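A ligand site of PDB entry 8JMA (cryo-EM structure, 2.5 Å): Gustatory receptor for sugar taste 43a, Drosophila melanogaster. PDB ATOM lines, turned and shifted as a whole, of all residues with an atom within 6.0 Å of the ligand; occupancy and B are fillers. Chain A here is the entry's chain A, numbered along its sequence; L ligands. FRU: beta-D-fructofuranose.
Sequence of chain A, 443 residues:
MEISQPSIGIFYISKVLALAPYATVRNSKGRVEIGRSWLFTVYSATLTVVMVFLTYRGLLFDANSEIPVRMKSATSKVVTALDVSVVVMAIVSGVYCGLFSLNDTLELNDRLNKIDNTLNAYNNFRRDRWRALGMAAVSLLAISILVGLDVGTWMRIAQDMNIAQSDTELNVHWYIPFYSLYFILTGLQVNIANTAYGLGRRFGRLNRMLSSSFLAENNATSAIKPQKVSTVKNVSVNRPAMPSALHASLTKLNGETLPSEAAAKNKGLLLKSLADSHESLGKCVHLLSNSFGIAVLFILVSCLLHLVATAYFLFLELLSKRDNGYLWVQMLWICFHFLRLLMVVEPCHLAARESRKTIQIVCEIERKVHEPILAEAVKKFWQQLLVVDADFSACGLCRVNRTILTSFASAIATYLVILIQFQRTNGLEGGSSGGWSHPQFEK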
ATOM      1  N   ARG A  70      -5.934  15.785   6.973  1.00  0.00           N
ATOM      2  CA  ARG A  70      -5.820  17.207   6.675  1.00  0.00           C
ATOM      3  C   ARG A  70      -5.906  17.520   5.190  1.00  0.00           C
ATOM      4  O   ARG A  70      -6.528  18.506   4.816  1.00  0.00           O
ATOM      5  CB  ARG A  70      -4.492  17.750   7.226  1.00  0.00           C
ATOM      6  CG  ARG A  70      -4.334  17.537   8.725  1.00  0.00           C
ATOM      7  CD  ARG A  70      -3.114  18.255   9.262  1.00  0.00           C
ATOM      8  NE  ARG A  70      -3.185  19.705   9.065  1.00  0.00           N
ATOM      9  CZ  ARG A  70      -2.431  20.590   9.695  1.00  0.00           C
ATOM     10  NH1 ARG A  70      -1.527  20.214  10.581  1.00  0.00           N
ATOM     11  NH2 ARG A  70      -2.590  21.881   9.431  1.00  0.00           N
ATOM     12  N   VAL A  79      -4.921  24.820   1.114  1.00  0.00           N
ATOM     13  CA  VAL A  79      -4.566  25.631   2.282  1.00  0.00           C
ATOM     14  C   VAL A  79      -3.486  24.945   3.106  1.00  0.00           C
ATOM     15  O   VAL A  79      -2.578  25.597   3.613  1.00  0.00           O
ATOM     16  CB  VAL A  79      -5.816  25.933   3.127  1.00  0.00           C
ATOM     17  CG1 VAL A  79      -5.415  26.626   4.409  1.00  0.00           C
ATOM     18  CG2 VAL A  79      -6.775  26.809   2.347  1.00  0.00           C
ATOM     19  N   ASP A  83       0.168  26.349   3.867  1.00  0.00           N
ATOM     20  CA  ASP A  83       0.588  26.456   5.264  1.00  0.00           C
ATOM     21  C   ASP A  83       1.951  25.800   5.470  1.00  0.00           C
ATOM     22  O   ASP A  83       2.824  26.368   6.134  1.00  0.00           O
ATOM     23  CB  ASP A  83      -0.466  25.818   6.155  1.00  0.00           C
ATOM     24  CG  ASP A  83      -0.242  26.067   7.626  1.00  0.00           C
ATOM     25  OD1 ASP A  83       0.920  25.973   8.082  1.00  0.00           O
ATOM     26  OD2 ASP A  83      -1.227  26.357   8.322  1.00  0.00           O
ATOM     27  N   VAL A  87       6.082  27.760   5.870  1.00  0.00           N
ATOM     28  CA  VAL A  87       7.037  27.373   6.904  1.00  0.00           C
ATOM     29  C   VAL A  87       8.319  26.847   6.266  1.00  0.00           C
ATOM     30  O   VAL A  87       9.424  27.165   6.710  1.00  0.00           O
ATOM     31  CB  VAL A  87       6.422  26.333   7.857  1.00  0.00           C
ATOM     32  CG1 VAL A  87       7.460  25.848   8.846  1.00  0.00           C
ATOM     33  CG2 VAL A  87       5.242  26.918   8.578  1.00  0.00           C
ATOM     34  N   ASP A 150      -1.913  20.912  19.011  1.00  0.00           N
ATOM     35  CA  ASP A 150      -2.266  20.599  17.629  1.00  0.00           C
ATOM     36  C   ASP A 150      -2.209  19.098  17.378  1.00  0.00           C
ATOM     37  O   ASP A 150      -3.105  18.535  16.737  1.00  0.00           O
ATOM     38  CB  ASP A 150      -1.326  21.338  16.686  1.00  0.00           C
ATOM     39  CG  ASP A 150      -1.976  21.692  15.370  1.00  0.00           C
ATOM     40  OD1 ASP A 150      -2.963  22.455  15.382  1.00  0.00           O
ATOM     41  OD2 ASP A 150      -1.500  21.207  14.323  1.00  0.00           O
ATOM     42  N   TRP A 154      -5.438  16.837  16.382  1.00  0.00           N
ATOM     43  CA  TRP A 154      -5.483  16.118  15.112  1.00  0.00           C
ATOM     44  C   TRP A 154      -5.508  14.617  15.333  1.00  0.00           C
ATOM     45  O   TRP A 154      -6.119  13.896  14.534  1.00  0.00           O
ATOM     46  CB  TRP A 154      -4.293  16.528  14.252  1.00  0.00           C
ATOM     47  CG  TRP A 154      -4.542  17.811  13.530  1.00  0.00           C
ATOM     48  CD1 TRP A 154      -3.876  18.988  13.690  1.00  0.00           C
ATOM     49  CD2 TRP A 154      -5.549  18.043  12.538  1.00  0.00           C
ATOM     50  NE1 TRP A 154      -4.400  19.938  12.854  1.00  0.00           N
ATOM     51  CE2 TRP A 154      -5.424  19.392  12.134  1.00  0.00           C
ATOM     52  CE3 TRP A 154      -6.534  17.258  11.943  1.00  0.00           C
ATOM     53  CZ2 TRP A 154      -6.249  19.961  11.180  1.00  0.00           C
ATOM     54  CZ3 TRP A 154      -7.352  17.820  10.992  1.00  0.00           C
ATOM     55  CH2 TRP A 154      -7.210  19.154  10.617  1.00  0.00           C
ATOM     56  N   PHE A 178       6.654  18.485   9.961  1.00  0.00           N
ATOM     57  CA  PHE A 178       6.143  19.850   9.873  1.00  0.00           C
ATOM     58  C   PHE A 178       6.296  20.582  11.202  1.00  0.00           C
ATOM     59  O   PHE A 178       6.690  21.752  11.234  1.00  0.00           O
ATOM     60  CB  PHE A 178       4.679  19.802   9.443  1.00  0.00           C
ATOM     61  CG  PHE A 178       4.036  21.158   9.320  1.00  0.00           C
ATOM     62  CD1 PHE A 178       4.705  22.202   8.717  1.00  0.00           C
ATOM     63  CD2 PHE A 178       2.767  21.373   9.805  1.00  0.00           C
ATOM     64  CE1 PHE A 178       4.122  23.438   8.607  1.00  0.00           C
ATOM     65  CE2 PHE A 178       2.184  22.609   9.695  1.00  0.00           C
ATOM     66  CZ  PHE A 178       2.859  23.646   9.095  1.00  0.00           C
ATOM     67  N   TYR A 179       6.018  19.899  12.310  1.00  0.00           N
ATOM     68  CA  TYR A 179       6.187  20.527  13.613  1.00  0.00           C
ATOM     69  C   TYR A 179       7.658  20.753  13.942  1.00  0.00           C
ATOM     70  O   TYR A 179       8.011  21.736  14.599  1.00  0.00           O
ATOM     71  CB  TYR A 179       5.514  19.673  14.685  1.00  0.00           C
ATOM     72  CG  TYR A 179       4.025  19.535  14.448  1.00  0.00           C
ATOM     73  CD1 TYR A 179       3.215  20.664  14.376  1.00  0.00           C
ATOM     74  CD2 TYR A 179       3.437  18.300  14.290  1.00  0.00           C
ATOM     75  CE1 TYR A 179       1.862  20.547  14.163  1.00  0.00           C
ATOM     76  CE2 TYR A 179       2.076  18.176  14.075  1.00  0.00           C
ATOM     77  CZ  TYR A 179       1.300  19.310  14.015  1.00  0.00           C
ATOM     78  OH  TYR A 179      -0.053  19.193  13.802  1.00  0.00           O
ATOM     79  N   TYR A 182       8.449  23.817  12.422  1.00  0.00           N
ATOM     80  CA  TYR A 182       7.944  24.916  13.241  1.00  0.00           C
ATOM     81  C   TYR A 182       8.918  25.261  14.361  1.00  0.00           C
ATOM     82  O   TYR A 182       9.111  26.432  14.695  1.00  0.00           O
ATOM     83  CB  TYR A 182       6.576  24.564  13.818  1.00  0.00           C
ATOM     84  CG  TYR A 182       5.471  25.374  13.195  1.00  0.00           C
ATOM     85  CD1 TYR A 182       5.374  26.728  13.417  1.00  0.00           C
ATOM     86  CD2 TYR A 182       4.535  24.768  12.385  1.00  0.00           C
ATOM     87  CE1 TYR A 182       4.365  27.474  12.846  1.00  0.00           C
ATOM     88  CE2 TYR A 182       3.527  25.500  11.806  1.00  0.00           C
ATOM     89  CZ  TYR A 182       3.440  26.853  12.042  1.00  0.00           C
ATOM     90  OH  TYR A 182       2.438  27.577  11.466  1.00  0.00           O
ATOM     91  N   HIS A 306      -0.313  32.549   7.267  1.00  0.00           N
ATOM     92  CA  HIS A 306      -0.819  31.780   8.400  1.00  0.00           C
ATOM     93  C   HIS A 306      -1.976  32.495   9.072  1.00  0.00           C
ATOM     94  O   HIS A 306      -2.946  31.848   9.460  1.00  0.00           O
ATOM     95  CB  HIS A 306       0.300  31.529   9.392  1.00  0.00           C
ATOM     96  CG  HIS A 306       1.165  30.371   9.038  1.00  0.00           C
ATOM     97  ND1 HIS A 306       2.512  30.330   9.331  1.00  0.00           N
ATOM     98  CD2 HIS A 306       0.883  29.197   8.428  1.00  0.00           C
ATOM     99  CE1 HIS A 306       3.018  29.187   8.911  1.00  0.00           C
ATOM    100  NE2 HIS A 306       2.051  28.480   8.346  1.00  0.00           N
ATOM    101  N   ALA A 309      -4.971  32.044   6.700  1.00  0.00           N
ATOM    102  CA  ALA A 309      -5.413  30.654   6.600  1.00  0.00           C
ATOM    103  C   ALA A 309      -6.020  30.165   7.911  1.00  0.00           C
ATOM    104  O   ALA A 309      -7.032  29.468   7.906  1.00  0.00           O
ATOM    105  CB  ALA A 309      -4.252  29.764   6.184  1.00  0.00           C
ATOM    106  N   THR A 310      -5.390  30.500   9.038  1.00  0.00           N
ATOM    107  CA  THR A 310      -5.908  30.072  10.331  1.00  0.00           C
ATOM    108  C   THR A 310      -7.231  30.745  10.639  1.00  0.00           C
ATOM    109  O   THR A 310      -8.148  30.102  11.173  1.00  0.00           O
ATOM    110  CB  THR A 310      -4.888  30.354  11.431  1.00  0.00           C
ATOM    111  OG1 THR A 310      -3.600  29.872  11.036  1.00  0.00           O
ATOM    112  CG2 THR A 310      -5.292  29.669  12.719  1.00  0.00           C
ATOM    113  N   PHE A 313      -9.819  28.906   8.469  1.00  0.00           N
ATOM    114  CA  PHE A 313     -10.190  27.610   9.025  1.00  0.00           C
ATOM    115  C   PHE A 313     -10.982  27.763  10.316  1.00  0.00           C
ATOM    116  O   PHE A 313     -11.884  26.964  10.585  1.00  0.00           O
ATOM    117  CB  PHE A 313      -8.951  26.758   9.272  1.00  0.00           C
ATOM    118  CG  PHE A 313      -8.433  26.043   8.053  1.00  0.00           C
ATOM    119  CD1 PHE A 313      -9.102  26.091   6.838  1.00  0.00           C
ATOM    120  CD2 PHE A 313      -7.264  25.293   8.125  1.00  0.00           C
ATOM    121  CE1 PHE A 313      -8.622  25.431   5.737  1.00  0.00           C
ATOM    122  CE2 PHE A 313      -6.778  24.626   7.027  1.00  0.00           C
ATOM    123  CZ  PHE A 313      -7.460  24.684   5.828  1.00  0.00           C
ATOM    124  N   TYR A 326     -10.842  22.177  18.509  1.00  0.00           N
ATOM    125  CA  TYR A 326     -10.268  22.710  17.278  1.00  0.00           C
ATOM    126  C   TYR A 326     -10.324  24.228  17.261  1.00  0.00           C
ATOM    127  O   TYR A 326      -9.340  24.882  16.898  1.00  0.00           O
ATOM    128  CB  TYR A 326     -10.992  22.137  16.059  1.00  0.00           C
ATOM    129  CG  TYR A 326     -10.348  22.477  14.735  1.00  0.00           C
ATOM    130  CD1 TYR A 326      -9.283  21.736  14.246  1.00  0.00           C
ATOM    131  CD2 TYR A 326     -10.813  23.540  13.971  1.00  0.00           C
ATOM    132  CE1 TYR A 326      -8.696  22.041  13.045  1.00  0.00           C
ATOM    133  CE2 TYR A 326     -10.231  23.853  12.767  1.00  0.00           C
ATOM    134  CZ  TYR A 326      -9.175  23.100  12.298  1.00  0.00           C
ATOM    135  OH  TYR A 326      -8.593  23.413  11.094  1.00  0.00           O
ATOM    136  N   GLN A 330      -7.096  26.669  17.147  1.00  0.00           N
ATOM    137  CA  GLN A 330      -6.943  27.616  16.051  1.00  0.00           C
ATOM    138  C   GLN A 330      -6.770  29.037  16.563  1.00  0.00           C
ATOM    139  O   GLN A 330      -5.972  29.807  16.015  1.00  0.00           O
ATOM    140  CB  GLN A 330      -8.134  27.530  15.113  1.00  0.00           C
ATOM    141  CG  GLN A 330      -8.241  26.218  14.345  1.00  0.00           C
ATOM    142  CD  GLN A 330      -6.983  25.885  13.571  1.00  0.00           C
ATOM    143  OE1 GLN A 330      -6.684  26.500  12.553  1.00  0.00           O
ATOM    144  NE2 GLN A 330      -6.244  24.900  14.060  1.00  0.00           N
ATOM    145  N   TRP A 333      -3.299  29.332  17.681  1.00  0.00           N
ATOM    146  CA  TRP A 333      -2.427  29.494  16.533  1.00  0.00           C
ATOM    147  C   TRP A 333      -2.456  30.931  16.012  1.00  0.00           C
ATOM    148  O   TRP A 333      -1.421  31.470  15.627  1.00  0.00           O
ATOM    149  CB  TRP A 333      -2.818  28.520  15.424  1.00  0.00           C
ATOM    150  CG  TRP A 333      -2.172  27.186  15.567  1.00  0.00           C
ATOM    151  CD1 TRP A 333      -2.797  25.997  15.807  1.00  0.00           C
ATOM    152  CD2 TRP A 333      -0.775  26.900  15.498  1.00  0.00           C
ATOM    153  NE1 TRP A 333      -1.871  24.998  15.884  1.00  0.00           N
ATOM    154  CE2 TRP A 333      -0.615  25.518  15.697  1.00  0.00           C
ATOM    155  CE3 TRP A 333       0.366  27.682  15.295  1.00  0.00           C
ATOM    156  CZ2 TRP A 333       0.623  24.899  15.695  1.00  0.00           C
ATOM    157  CZ3 TRP A 333       1.594  27.063  15.278  1.00  0.00           C
ATOM    158  CH2 TRP A 333       1.721  25.686  15.486  1.00  0.00           C
ATOM    159  N   ILE A 334      -3.641  31.534  15.971  1.00  0.00           N
ATOM    160  CA  ILE A 334      -3.737  32.928  15.537  1.00  0.00           C
ATOM    161  C   ILE A 334      -2.943  33.830  16.478  1.00  0.00           C
ATOM    162  O   ILE A 334      -2.213  34.722  16.041  1.00  0.00           O
ATOM    163  CB  ILE A 334      -5.210  33.362  15.456  1.00  0.00           C
ATOM    164  CG1 ILE A 334      -5.832  32.870  14.146  1.00  0.00           C
ATOM    165  CG2 ILE A 334      -5.333  34.880  15.542  1.00  0.00           C
ATOM    166  CD1 ILE A 334      -7.333  32.858  14.157  1.00  0.00           C
ATOM    167  N   HIS A 337       0.782  33.325  15.757  1.00  0.00           N
ATOM    168  CA  HIS A 337       1.229  33.958  14.523  1.00  0.00           C
ATOM    169  C   HIS A 337       1.293  35.474  14.677  1.00  0.00           C
ATOM    170  O   HIS A 337       2.219  36.110  14.178  1.00  0.00           O
ATOM    171  CB  HIS A 337       0.313  33.554  13.377  1.00  0.00           C
ATOM    172  CG  HIS A 337       0.404  32.107  13.026  1.00  0.00           C
ATOM    173  ND1 HIS A 337       1.600  31.456  12.819  1.00  0.00           N
ATOM    174  CD2 HIS A 337      -0.557  31.164  12.862  1.00  0.00           C
ATOM    175  CE1 HIS A 337       1.379  30.192  12.539  1.00  0.00           C
ATOM    176  NE2 HIS A 337       0.070  29.986  12.555  1.00  0.00           N
HETATM  177  C1  FRU L   1      -0.078  23.887  12.430  1.00  0.00           C
HETATM  178  C2  FRU L   1      -0.946  24.758  11.523  1.00  0.00           C
HETATM  179  C3  FRU L   1      -0.547  26.182  11.625  1.00  0.00           C
HETATM  180  C4  FRU L   1      -1.778  26.941  11.497  1.00  0.00           C
HETATM  181  C5  FRU L   1      -2.863  26.061  12.019  1.00  0.00           C
HETATM  182  C6  FRU L   1      -4.088  26.185  11.185  1.00  0.00           C
HETATM  183  O1  FRU L   1      -0.162  22.554  12.004  1.00  0.00           O
HETATM  184  O2  FRU L   1      -0.844  24.327  10.230  1.00  0.00           O
HETATM  185  O3  FRU L   1       0.367  26.537  10.555  1.00  0.00           O
HETATM  186  O4  FRU L   1      -1.688  28.157  12.291  1.00  0.00           O
HETATM  187  O5  FRU L   1      -2.354  24.664  11.961  1.00  0.00           O
HETATM  188  O6  FRU L   1      -3.792  25.951   9.844  1.00  0.00           O
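NE2 of His 306 sits close to OH of Tyr 182 (3.3 Å).
NE2 of His 306 is in hydrogen-bond range of OD1 of Asp 83, at 2.8 Å.
The side-chain hydroxyl (OG1) of Thr 310 is in hydrogen-bond range of the backbone carbonyl oxygen (O) of His 306, 2.6 Å away.
The guanidinium group (NH1) of Arg 70 is in salt-bridge range of the side-chain carboxylate (OD2) of Asp 150, 3.9 Å away.
OD1 of Asp 150 sits at hydrogen-bond distance from NE1 of Trp 333 (2.8 Å).
The side-chain carboxylate (OD2) of Asp 150 is in hydrogen-bond range of the side-chain hydroxyl (OH) of Tyr 179, 2.5 Å away.
The indole nitrogen (NE1) of Trp 154 lies close to the side-chain carboxylate (OD2) of Asp 150 (3.5 Å).
O3 of the ligand is in hydrogen-bond range of OH of Tyr 182, 2.5 Å away.
An oxygen (O4) of the ligand is in hydrogen-bond range of a ring nitrogen (NE2) of His 337, at 2.6 Å.
The side-chain carboxylate of Asp 83 sits at hydrogen-bond distance from an oxygen (O3) of the ligand, at 2.6 Å.
The side-chain hydroxyl (OG1) of Thr 310 lies within hydrogen-bond range of an oxygen (O4) of the ligand (2.9 Å).
The side-chain carboxylate (OD2) of Asp 150 sits at hydrogen-bond distance from an oxygen (O1) of the ligand.
An oxygen (O1) of the ligand lies within hydrogen-bond range of the guanidinium group of Arg 70 (3.1 Å).
O3 of the ligand sits at hydrogen-bond distance from NE2 of His 306 (3.4 Å).
Merely in contact with the ligand: Phe 178 (3.3 Å), Tyr 179 (3.6 Å), Phe 313 (3.9 Å), Gln 330 (3.0 Å) and Trp 333 (3.4 Å).
Hydrophobic or aromatic side chains within 4 Å of the ligand: Phe 178, Tyr 179, Tyr 182, His 306, Phe 313, Trp 333 and His 337.
Of the 18 residues printed, 12 come within 4 Å of the ligand.
The nearest printed residue that does not touch the ligand is Trp 154 (5.1 Å).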
